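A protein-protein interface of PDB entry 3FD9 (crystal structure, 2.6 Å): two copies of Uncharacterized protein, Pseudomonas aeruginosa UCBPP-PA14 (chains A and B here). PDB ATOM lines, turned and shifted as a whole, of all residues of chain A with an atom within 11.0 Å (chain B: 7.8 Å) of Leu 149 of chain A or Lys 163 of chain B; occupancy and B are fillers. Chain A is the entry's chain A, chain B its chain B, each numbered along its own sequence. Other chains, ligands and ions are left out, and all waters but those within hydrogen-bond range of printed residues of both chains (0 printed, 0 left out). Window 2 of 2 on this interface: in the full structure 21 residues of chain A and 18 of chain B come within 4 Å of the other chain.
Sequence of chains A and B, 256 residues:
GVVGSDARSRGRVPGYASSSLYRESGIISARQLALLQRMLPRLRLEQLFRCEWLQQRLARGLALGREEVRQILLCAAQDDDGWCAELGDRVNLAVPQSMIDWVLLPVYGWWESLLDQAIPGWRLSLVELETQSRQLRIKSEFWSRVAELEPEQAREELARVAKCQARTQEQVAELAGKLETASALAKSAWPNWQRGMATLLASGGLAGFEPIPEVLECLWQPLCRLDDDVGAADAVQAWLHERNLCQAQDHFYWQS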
ATOM      1  N   GLU A 141      28.225  10.752  34.809  1.00  0.00           N
ATOM      2  CA  GLU A 141      28.330  10.334  33.418  1.00  0.00           C
ATOM      3  C   GLU A 141      26.995   9.756  32.975  1.00  0.00           C
ATOM      4  O   GLU A 141      26.654   9.770  31.792  1.00  0.00           O
ATOM      5  CB  GLU A 141      29.426   9.280  33.255  1.00  0.00           C
ATOM      6  CG  GLU A 141      30.841   9.822  33.367  1.00  0.00           C
ATOM      7  CD  GLU A 141      31.274  10.576  32.125  1.00  0.00           C
ATOM      8  OE1 GLU A 141      30.448  10.733  31.200  1.00  0.00           O
ATOM      9  OE2 GLU A 141      32.445  11.008  32.075  1.00  0.00           O
ATOM     10  N   PHE A 142      26.247   9.242  33.944  1.00  0.00           N
ATOM     11  CA  PHE A 142      24.921   8.705  33.688  1.00  0.00           C
ATOM     12  C   PHE A 142      23.930   9.823  33.384  1.00  0.00           C
ATOM     13  O   PHE A 142      23.268   9.808  32.349  1.00  0.00           O
ATOM     14  CB  PHE A 142      24.436   7.890  34.889  1.00  0.00           C
ATOM     15  CG  PHE A 142      23.032   7.373  34.745  1.00  0.00           C
ATOM     16  CD1 PHE A 142      22.796   6.075  34.324  1.00  0.00           C
ATOM     17  CD2 PHE A 142      21.944   8.191  35.023  1.00  0.00           C
ATOM     18  CE1 PHE A 142      21.502   5.600  34.188  1.00  0.00           C
ATOM     19  CE2 PHE A 142      20.651   7.721  34.888  1.00  0.00           C
ATOM     20  CZ  PHE A 142      20.431   6.425  34.469  1.00  0.00           C
ATOM     21  N   TRP A 143      23.830  10.789  34.290  1.00  0.00           N
ATOM     22  CA  TRP A 143      22.856  11.863  34.148  1.00  0.00           C
ATOM     23  C   TRP A 143      23.265  12.896  33.104  1.00  0.00           C
ATOM     24  O   TRP A 143      22.508  13.820  32.805  1.00  0.00           O
ATOM     25  CB  TRP A 143      22.577  12.526  35.500  1.00  0.00           C
ATOM     26  CG  TRP A 143      21.671  11.703  36.366  1.00  0.00           C
ATOM     27  CD1 TRP A 143      22.043  10.744  37.264  1.00  0.00           C
ATOM     28  CD2 TRP A 143      20.240  11.754  36.406  1.00  0.00           C
ATOM     29  NE1 TRP A 143      20.933  10.198  37.862  1.00  0.00           N
ATOM     30  CE2 TRP A 143      19.811  10.802  37.352  1.00  0.00           C
ATOM     31  CE3 TRP A 143      19.275  12.515  35.734  1.00  0.00           C
ATOM     32  CZ2 TRP A 143      18.465  10.588  37.645  1.00  0.00           C
ATOM     33  CZ3 TRP A 143      17.938  12.303  36.026  1.00  0.00           C
ATOM     34  CH2 TRP A 143      17.545  11.348  36.973  1.00  0.00           C
ATOM     35  N   SER A 144      24.462  12.734  32.551  1.00  0.00           N
ATOM     36  CA  SER A 144      24.888  13.547  31.419  1.00  0.00           C
ATOM     37  C   SER A 144      24.256  13.005  30.146  1.00  0.00           C
ATOM     38  O   SER A 144      23.845  13.764  29.265  1.00  0.00           O
ATOM     39  CB  SER A 144      26.412  13.539  31.288  1.00  0.00           C
ATOM     40  OG  SER A 144      27.016  14.278  32.335  1.00  0.00           O
ATOM     41  N   ARG A 145      24.183  11.681  30.061  1.00  0.00           N
ATOM     42  CA  ARG A 145      23.566  11.005  28.929  1.00  0.00           C
ATOM     43  C   ARG A 145      22.055  11.173  28.968  1.00  0.00           C
ATOM     44  O   ARG A 145      21.370  10.965  27.965  1.00  0.00           O
ATOM     45  CB  ARG A 145      23.921   9.520  28.947  1.00  0.00           C
ATOM     46  CG  ARG A 145      25.409   9.243  28.862  1.00  0.00           C
ATOM     47  CD  ARG A 145      25.927   9.453  27.454  1.00  0.00           C
ATOM     48  NE  ARG A 145      27.372   9.271  27.375  1.00  0.00           N
ATOM     49  CZ  ARG A 145      28.070   9.328  26.247  1.00  0.00           C
ATOM     50  NH1 ARG A 145      27.450   9.557  25.097  1.00  0.00           N
ATOM     51  NH2 ARG A 145      29.385   9.153  26.269  1.00  0.00           N
ATOM     52  N   VAL A 146      21.540  11.542  30.135  1.00  0.00           N
ATOM     53  CA  VAL A 146      20.112  11.765  30.300  1.00  0.00           C
ATOM     54  C   VAL A 146      19.783  13.244  30.122  1.00  0.00           C
ATOM     55  O   VAL A 146      18.703  13.595  29.655  1.00  0.00           O
ATOM     56  CB  VAL A 146      19.625  11.281  31.680  1.00  0.00           C
ATOM     57  CG1 VAL A 146      18.173  11.674  31.908  1.00  0.00           C
ATOM     58  CG2 VAL A 146      19.798   9.774  31.804  1.00  0.00           C
ATOM     59  N   ALA A 147      20.731  14.104  30.483  1.00  0.00           N
ATOM     60  CA  ALA A 147      20.543  15.549  30.393  1.00  0.00           C
ATOM     61  C   ALA A 147      20.034  15.996  29.023  1.00  0.00           C
ATOM     62  O   ALA A 147      19.397  17.046  28.900  1.00  0.00           O
ATOM     63  CB  ALA A 147      21.841  16.270  30.738  1.00  0.00           C
ATOM     64  N   GLU A 148      20.318  15.197  27.998  1.00  0.00           N
ATOM     65  CA  GLU A 148      19.927  15.528  26.629  1.00  0.00           C
ATOM     66  C   GLU A 148      18.442  15.287  26.385  1.00  0.00           C
ATOM     67  O   GLU A 148      17.772  16.092  25.738  1.00  0.00           O
ATOM     68  CB  GLU A 148      20.755  14.723  25.626  1.00  0.00           C
ATOM     69  CG  GLU A 148      20.621  13.216  25.786  1.00  0.00           C
ATOM     70  CD  GLU A 148      21.619  12.448  24.941  1.00  0.00           C
ATOM     71  OE1 GLU A 148      22.205  13.054  24.020  1.00  0.00           O
ATOM     72  OE2 GLU A 148      21.818  11.241  25.199  1.00  0.00           O
ATOM     73  N   LEU A 149      17.932  14.177  26.910  1.00  0.00           N
ATOM     74  CA  LEU A 149      16.534  13.807  26.722  1.00  0.00           C
ATOM     75  C   LEU A 149      15.664  14.360  27.851  1.00  0.00           C
ATOM     76  O   LEU A 149      14.536  14.801  27.623  1.00  0.00           O
ATOM     77  CB  LEU A 149      16.402  12.286  26.634  1.00  0.00           C
ATOM     78  CG  LEU A 149      15.105  11.726  26.048  1.00  0.00           C
ATOM     79  CD1 LEU A 149      14.693  12.490  24.795  1.00  0.00           C
ATOM     80  CD2 LEU A 149      15.270  10.247  25.750  1.00  0.00           C
ATOM     81  N   GLU A 150      16.199  14.330  29.066  1.00  0.00           N
ATOM     82  CA  GLU A 150      15.538  14.922  30.222  1.00  0.00           C
ATOM     83  C   GLU A 150      16.340  16.122  30.711  1.00  0.00           C
ATOM     84  O   GLU A 150      17.031  16.039  31.726  1.00  0.00           O
ATOM     85  CB  GLU A 150      15.399  13.899  31.353  1.00  0.00           C
ATOM     86  CG  GLU A 150      14.539  12.690  31.013  1.00  0.00           C
ATOM     87  CD  GLU A 150      14.474  11.680  32.148  1.00  0.00           C
ATOM     88  OE1 GLU A 150      14.990  11.980  33.247  1.00  0.00           O
ATOM     89  OE2 GLU A 150      13.907  10.586  31.941  1.00  0.00           O
ATOM     90  N   PRO A 151      16.255  17.243  29.983  1.00  0.00           N
ATOM     91  CA  PRO A 151      17.017  18.443  30.336  1.00  0.00           C
ATOM     92  C   PRO A 151      16.604  18.986  31.698  1.00  0.00           C
ATOM     93  O   PRO A 151      17.462  19.267  32.535  1.00  0.00           O
ATOM     94  CB  PRO A 151      16.632  19.441  29.238  1.00  0.00           C
ATOM     95  CG  PRO A 151      16.086  18.607  28.121  1.00  0.00           C
ATOM     96  CD  PRO A 151      15.419  17.453  28.789  1.00  0.00           C
ATOM     97  N   GLU A 152      15.300  19.119  31.914  1.00  0.00           N
ATOM     98  CA  GLU A 152      14.780  19.746  33.126  1.00  0.00           C
ATOM     99  C   GLU A 152      15.094  18.973  34.413  1.00  0.00           C
ATOM    100  O   GLU A 152      15.775  19.490  35.300  1.00  0.00           O
ATOM    101  CB  GLU A 152      13.272  20.025  32.997  1.00  0.00           C
ATOM    102  CG  GLU A 152      12.358  18.802  33.059  1.00  0.00           C
ATOM    103  CD  GLU A 152      12.586  17.826  31.919  1.00  0.00           C
ATOM    104  OE1 GLU A 152      11.755  17.794  30.987  1.00  0.00           O
ATOM    105  OE2 GLU A 152      13.595  17.088  31.953  1.00  0.00           O
ATOM    106  N   GLN A 153      14.610  17.739  34.509  1.00  0.00           N
ATOM    107  CA  GLN A 153      14.750  16.956  35.734  1.00  0.00           C
ATOM    108  C   GLN A 153      16.161  16.408  35.926  1.00  0.00           C
ATOM    109  O   GLN A 153      16.363  15.431  36.649  1.00  0.00           O
ATOM    110  CB  GLN A 153      13.732  15.812  35.763  1.00  0.00           C
ATOM    111  CG  GLN A 153      12.285  16.270  35.883  1.00  0.00           C
ATOM    112  CD  GLN A 153      11.960  16.842  37.253  1.00  0.00           C
ATOM    113  OE1 GLN A 153      12.687  16.616  38.222  1.00  0.00           O
ATOM    114  NE2 GLN A 153      10.862  17.586  37.339  1.00  0.00           N
ATOM    115  N   ALA A 154      17.133  17.040  35.277  1.00  0.00           N
ATOM    116  CA  ALA A 154      18.527  16.630  35.399  1.00  0.00           C
ATOM    117  C   ALA A 154      19.330  17.687  36.145  1.00  0.00           C
ATOM    118  O   ALA A 154      20.410  17.410  36.662  1.00  0.00           O
ATOM    119  CB  ALA A 154      19.131  16.370  34.026  1.00  0.00           C
ATOM    120  N   ARG A 155      18.792  18.900  36.201  1.00  0.00           N
ATOM    121  CA  ARG A 155      19.462  19.998  36.884  1.00  0.00           C
ATOM    122  C   ARG A 155      19.437  19.768  38.391  1.00  0.00           C
ATOM    123  O   ARG A 155      20.136  20.441  39.146  1.00  0.00           O
ATOM    124  CB  ARG A 155      18.783  21.329  36.554  1.00  0.00           C
ATOM    125  CG  ARG A 155      17.820  21.812  37.629  1.00  0.00           C
ATOM    126  CD  ARG A 155      17.060  23.054  37.195  1.00  0.00           C
ATOM    127  NE  ARG A 155      15.711  22.743  36.730  1.00  0.00           N
ATOM    128  CZ  ARG A 155      15.400  22.424  35.478  1.00  0.00           C
ATOM    129  NH1 ARG A 155      16.345  22.367  34.549  1.00  0.00           N
ATOM    130  NH2 ARG A 155      14.141  22.159  35.156  1.00  0.00           N
ATOM    131  N   LEU B 136      21.612   1.445  32.077  1.00  0.00           N
ATOM    132  CA  LEU B 136      20.205   1.648  31.741  1.00  0.00           C
ATOM    133  C   LEU B 136      19.373   0.382  31.918  1.00  0.00           C
ATOM    134  O   LEU B 136      18.202   0.453  32.279  1.00  0.00           O
ATOM    135  CB  LEU B 136      20.055   2.185  30.311  1.00  0.00           C
ATOM    136  CG  LEU B 136      19.930   3.703  30.149  1.00  0.00           C
ATOM    137  CD1 LEU B 136      20.874   4.446  31.081  1.00  0.00           C
ATOM    138  CD2 LEU B 136      20.168   4.109  28.701  1.00  0.00           C
ATOM    139  N   GLU B 157       9.185   6.062  36.347  1.00  0.00           N
ATOM    140  CA  GLU B 157      10.626   5.975  36.126  1.00  0.00           C
ATOM    141  C   GLU B 157      10.970   5.134  34.903  1.00  0.00           C
ATOM    142  O   GLU B 157      11.890   5.457  34.153  1.00  0.00           O
ATOM    143  CB  GLU B 157      11.307   5.384  37.360  1.00  0.00           C
ATOM    144  CG  GLU B 157      11.018   6.138  38.645  1.00  0.00           C
ATOM    145  CD  GLU B 157      11.740   7.466  38.715  1.00  0.00           C
ATOM    146  OE1 GLU B 157      12.715   7.657  37.954  1.00  0.00           O
ATOM    147  OE2 GLU B 157      11.337   8.319  39.535  1.00  0.00           O
ATOM    148  N   LEU B 158      10.229   4.047  34.716  1.00  0.00           N
ATOM    149  CA  LEU B 158      10.438   3.160  33.583  1.00  0.00           C
ATOM    150  C   LEU B 158      10.230   3.899  32.263  1.00  0.00           C
ATOM    151  O   LEU B 158      11.030   3.776  31.340  1.00  0.00           O
ATOM    152  CB  LEU B 158       9.496   1.958  33.671  1.00  0.00           C
ATOM    153  CG  LEU B 158       9.839   0.898  34.719  1.00  0.00           C
ATOM    154  CD1 LEU B 158       8.713  -0.121  34.849  1.00  0.00           C
ATOM    155  CD2 LEU B 158      11.158   0.214  34.380  1.00  0.00           C
ATOM    156  N   ALA B 159       9.147   4.661  32.175  1.00  0.00           N
ATOM    157  CA  ALA B 159       8.893   5.459  30.985  1.00  0.00           C
ATOM    158  C   ALA B 159      10.059   6.408  30.753  1.00  0.00           C
ATOM    159  O   ALA B 159      10.446   6.667  29.616  1.00  0.00           O
ATOM    160  CB  ALA B 159       7.591   6.232  31.129  1.00  0.00           C
ATOM    161  N   ARG B 160      10.623   6.914  31.845  1.00  0.00           N
ATOM    162  CA  ARG B 160      11.734   7.853  31.774  1.00  0.00           C
ATOM    163  C   ARG B 160      12.976   7.212  31.157  1.00  0.00           C
ATOM    164  O   ARG B 160      13.552   7.746  30.208  1.00  0.00           O
ATOM    165  CB  ARG B 160      12.059   8.398  33.167  1.00  0.00           C
ATOM    166  CG  ARG B 160      10.979   9.296  33.760  1.00  0.00           C
ATOM    167  CD  ARG B 160      10.998  10.682  33.127  1.00  0.00           C
ATOM    168  NE  ARG B 160      10.036  11.591  33.749  1.00  0.00           N
ATOM    169  CZ  ARG B 160       8.930  12.036  33.156  1.00  0.00           C
ATOM    170  NH1 ARG B 160       8.638  11.659  31.918  1.00  0.00           N
ATOM    171  NH2 ARG B 160       8.115  12.862  33.802  1.00  0.00           N
ATOM    172  N   VAL B 161      13.385   6.068  31.701  1.00  0.00           N
ATOM    173  CA  VAL B 161      14.578   5.375  31.219  1.00  0.00           C
ATOM    174  C   VAL B 161      14.338   4.696  29.872  1.00  0.00           C
ATOM    175  O   VAL B 161      15.264   4.520  29.081  1.00  0.00           O
ATOM    176  CB  VAL B 161      15.094   4.328  32.235  1.00  0.00           C
ATOM    177  CG1 VAL B 161      15.367   4.982  33.578  1.00  0.00           C
ATOM    178  CG2 VAL B 161      14.101   3.190  32.382  1.00  0.00           C
ATOM    179  N   ALA B 162      13.093   4.313  29.615  1.00  0.00           N
ATOM    180  CA  ALA B 162      12.744   3.691  28.347  1.00  0.00           C
ATOM    181  C   ALA B 162      13.155   4.606  27.201  1.00  0.00           C
ATOM    182  O   ALA B 162      13.730   4.162  26.211  1.00  0.00           O
ATOM    183  CB  ALA B 162      11.253   3.398  28.289  1.00  0.00           C
ATOM    184  N   LYS B 163      12.863   5.893  27.350  1.00  0.00           N
ATOM    185  CA  LYS B 163      13.195   6.876  26.328  1.00  0.00           C
ATOM    186  C   LYS B 163      14.707   6.949  26.110  1.00  0.00           C
ATOM    187  O   LYS B 163      15.173   7.124  24.985  1.00  0.00           O
ATOM    188  CB  LYS B 163      12.657   8.255  26.721  1.00  0.00           C
ATOM    189  CG  LYS B 163      11.167   8.304  27.034  1.00  0.00           C
ATOM    190  CD  LYS B 163      10.311   8.266  25.776  1.00  0.00           C
ATOM    191  CE  LYS B 163       8.851   8.556  26.103  1.00  0.00           C
ATOM    192  NZ  LYS B 163       8.019   8.717  24.882  1.00  0.00           N
ATOM    193  N   CYS B 164      15.467   6.810  27.192  1.00  0.00           N
ATOM    194  CA  CYS B 164      16.918   6.951  27.130  1.00  0.00           C
ATOM    195  C   CYS B 164      17.593   5.836  26.342  1.00  0.00           C
ATOM    196  O   CYS B 164      18.428   6.098  25.478  1.00  0.00           O
ATOM    197  CB  CYS B 164      17.507   7.019  28.537  1.00  0.00           C
ATOM    198  SG  CYS B 164      16.981   8.461  29.484  1.00  0.00           S
ATOM    199  N   GLN B 165      17.241   4.592  26.645  1.00  0.00           N
ATOM    200  CA  GLN B 165      17.842   3.454  25.965  1.00  0.00           C
ATOM    201  C   GLN B 165      17.465   3.425  24.489  1.00  0.00           C
ATOM    202  O   GLN B 165      18.173   2.841  23.671  1.00  0.00           O
ATOM    203  CB  GLN B 165      17.458   2.143  26.656  1.00  0.00           C
ATOM    204  CG  GLN B 165      16.031   2.100  27.171  1.00  0.00           C
ATOM    205  CD  GLN B 165      15.890   1.245  28.421  1.00  0.00           C
ATOM    206  OE1 GLN B 165      16.860   0.637  28.887  1.00  0.00           O
ATOM    207  NE2 GLN B 165      14.680   1.203  28.977  1.00  0.00           N
ATOM    208  N   ALA B 166      16.349   4.065  24.154  1.00  0.00           N
ATOM    209  CA  ALA B 166      15.917   4.176  22.765  1.00  0.00           C
ATOM    210  C   ALA B 166      16.856   5.100  22.000  1.00  0.00           C
ATOM    211  O   ALA B 166      17.300   4.776  20.899  1.00  0.00           O
ATOM    212  CB  ALA B 166      14.484   4.689  22.689  1.00  0.00           C
ATOM    213  N   ARG B 167      17.152   6.252  22.593  1.00  0.00           N
ATOM    214  CA  ARG B 167      18.096   7.192  22.008  1.00  0.00           C
ATOM    215  C   ARG B 167      19.508   6.624  22.038  1.00  0.00           C
ATOM    216  O   ARG B 167      20.242   6.706  21.055  1.00  0.00           O
ATOM    217  CB  ARG B 167      18.053   8.531  22.747  1.00  0.00           C
ATOM    218  CG  ARG B 167      19.236   9.434  22.436  1.00  0.00           C
ATOM    219  CD  ARG B 167      19.047  10.832  23.002  1.00  0.00           C
ATOM    220  NE  ARG B 167      18.037  11.592  22.268  1.00  0.00           N
ATOM    221  CZ  ARG B 167      18.273  12.271  21.149  1.00  0.00           C
ATOM    222  NH1 ARG B 167      19.493  12.287  20.623  1.00  0.00           N
ATOM    223  NH2 ARG B 167      17.288  12.933  20.552  1.00  0.00           N
ATOM    224  N   THR B 168      19.892   6.046  23.171  1.00  0.00           N
ATOM    225  CA  THR B 168      21.215   5.455  23.297  1.00  0.00           C
ATOM    226  C   THR B 168      21.431   4.385  22.235  1.00  0.00           C
ATOM    227  O   THR B 168      22.516   4.275  21.672  1.00  0.00           O
ATOM    228  CB  THR B 168      21.446   4.857  24.693  1.00  0.00           C
ATOM    229  OG1 THR B 168      21.639   5.915  25.641  1.00  0.00           O
ATOM    230  CG2 THR B 168      22.678   3.972  24.688  1.00  0.00           C
ATOM    231  N   GLN B 169      20.398   3.599  21.956  1.00  0.00           N
ATOM    232  CA  GLN B 169      20.486   2.588  20.908  1.00  0.00           C
ATOM    233  C   GLN B 169      20.692   3.217  19.538  1.00  0.00           C
ATOM    234  O   GLN B 169      21.424   2.684  18.709  1.00  0.00           O
ATOM    235  CB  GLN B 169      19.244   1.695  20.898  1.00  0.00           C
ATOM    236  CG  GLN B 169      19.502   0.277  21.382  1.00  0.00           C
ATOM    237  CD  GLN B 169      20.302   0.236  22.670  1.00  0.00           C
ATOM    238  OE1 GLN B 169      19.810   0.620  23.733  1.00  0.00           O
ATOM    239  NE2 GLN B 169      21.542  -0.239  22.582  1.00  0.00           N
ATOM    240  N   GLU B 170      20.047   4.355  19.307  1.00  0.00           N
ATOM    241  CA  GLU B 170      20.132   5.023  18.016  1.00  0.00           C
ATOM    242  C   GLU B 170      21.495   5.662  17.808  1.00  0.00           C
ATOM    243  O   GLU B 170      22.071   5.579  16.721  1.00  0.00           O
ATOM    244  CB  GLU B 170      19.030   6.072  17.871  1.00  0.00           C
ATOM    245  CG  GLU B 170      17.624   5.498  17.911  1.00  0.00           C
ATOM    246  CD  GLU B 170      16.582   6.477  17.406  1.00  0.00           C
ATOM    247  OE1 GLU B 170      16.775   7.033  16.304  1.00  0.00           O
ATOM    248  OE2 GLU B 170      15.570   6.684  18.111  1.00  0.00           O
ATOM    249  N   GLN B 171      22.008   6.301  18.852  1.00  0.00           N
ATOM    250  CA  GLN B 171      23.320   6.925  18.781  1.00  0.00           C
ATOM    251  C   GLN B 171      24.372   5.877  18.448  1.00  0.00           C
ATOM    252  O   GLN B 171      25.327   6.152  17.728  1.00  0.00           O
ATOM    253  CB  GLN B 171      23.663   7.614  20.101  1.00  0.00           C
ATOM    254  CG  GLN B 171      22.913   8.909  20.342  1.00  0.00           C
ATOM    255  CD  GLN B 171      23.287   9.562  21.663  1.00  0.00           C
ATOM    256  OE1 GLN B 171      22.745  10.605  22.029  1.00  0.00           O
ATOM    257  NE2 GLN B 171      24.217   8.948  22.386  1.00  0.00           N
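The side-chain hydroxyl (OG1) of Thr 168 of chain B is in hydrogen-bond range of the backbone carbonyl oxygen (O) of Cys 164 of chain B (3.2 Å). O of Arg 160 of chain B sits at hydrogen-bond distance from SG of Cys 164 of chain B, at 3.6 Å.
The side-chain amide oxygen of Gln 171 of chain B lies close to the side-chain carboxylate of Glu 148 of chain A, at 3.2 Å. The backbone carbonyl oxygen (O) of Arg 160 of chain B lies close to the side-chain carboxylate (OE2) of Glu 150 of chain A (3.3 Å).
No position is printed for both chains.
Hydrophobic or aromatic side chains of chain A within 4 Å of the printed part of chain B: Phe 142, Val 146 and Leu 149. Of the 16 printed residues of chain B, 6 touch a printed residue of chain A. Printed residues of chain B that touch a printed residue of chain A: Leu 136, Arg 160, Lys 163, Cys 164, Arg 167 and Gln 171. Hydrophobic or aromatic side chains of chain B that line the printed part of chain A: Leu 136. Among the printed residues, 7 pairs touch across the chains.
Of the printed residues of chain B, Glu 148 of chain A touches Arg 167 and Gln 171. Of chain B, only Lys 163 (3.2 Å) and Cys 164 (3.7 Å) come within 4 Å of Leu 149 of chain A. Of the printed residues of chain B, Glu 150 of chain A touches Arg 160. Ala 159 of chain B touches none of the printed residues of chain A. Of the printed residues of chain A, Arg 160 of chain B touches Glu 150. Of chain A, only Leu 149 (3.2 Å) comes within 4 Å of Lys 163 of chain B. Of chain A, only Val 146 (3.9 Å) and Leu 149 (3.7 Å) come within 4 Å of Cys 164 of chain B. Gln 165 of chain B touches none of the printed residues of chain A. Of the printed residues of chain A, Arg 167 of chain B touches Glu 148 (3.6 Å). Glu 170 of chain B touches none of the printed residues of chain A.
Phe 142 of chain A touches Leu 136 of chain B (CE1 to CD1, 3.4 Å). Cys 164 of chain B touches Val 146 of chain A. Glu 148 of chain A touches Arg 167 of chain B. CD2 of Leu 149 of chain A touches O of Lys 163 of chain B, 3.2 Å away. Leu 149 of chain A touches Cys 164 of chain B.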
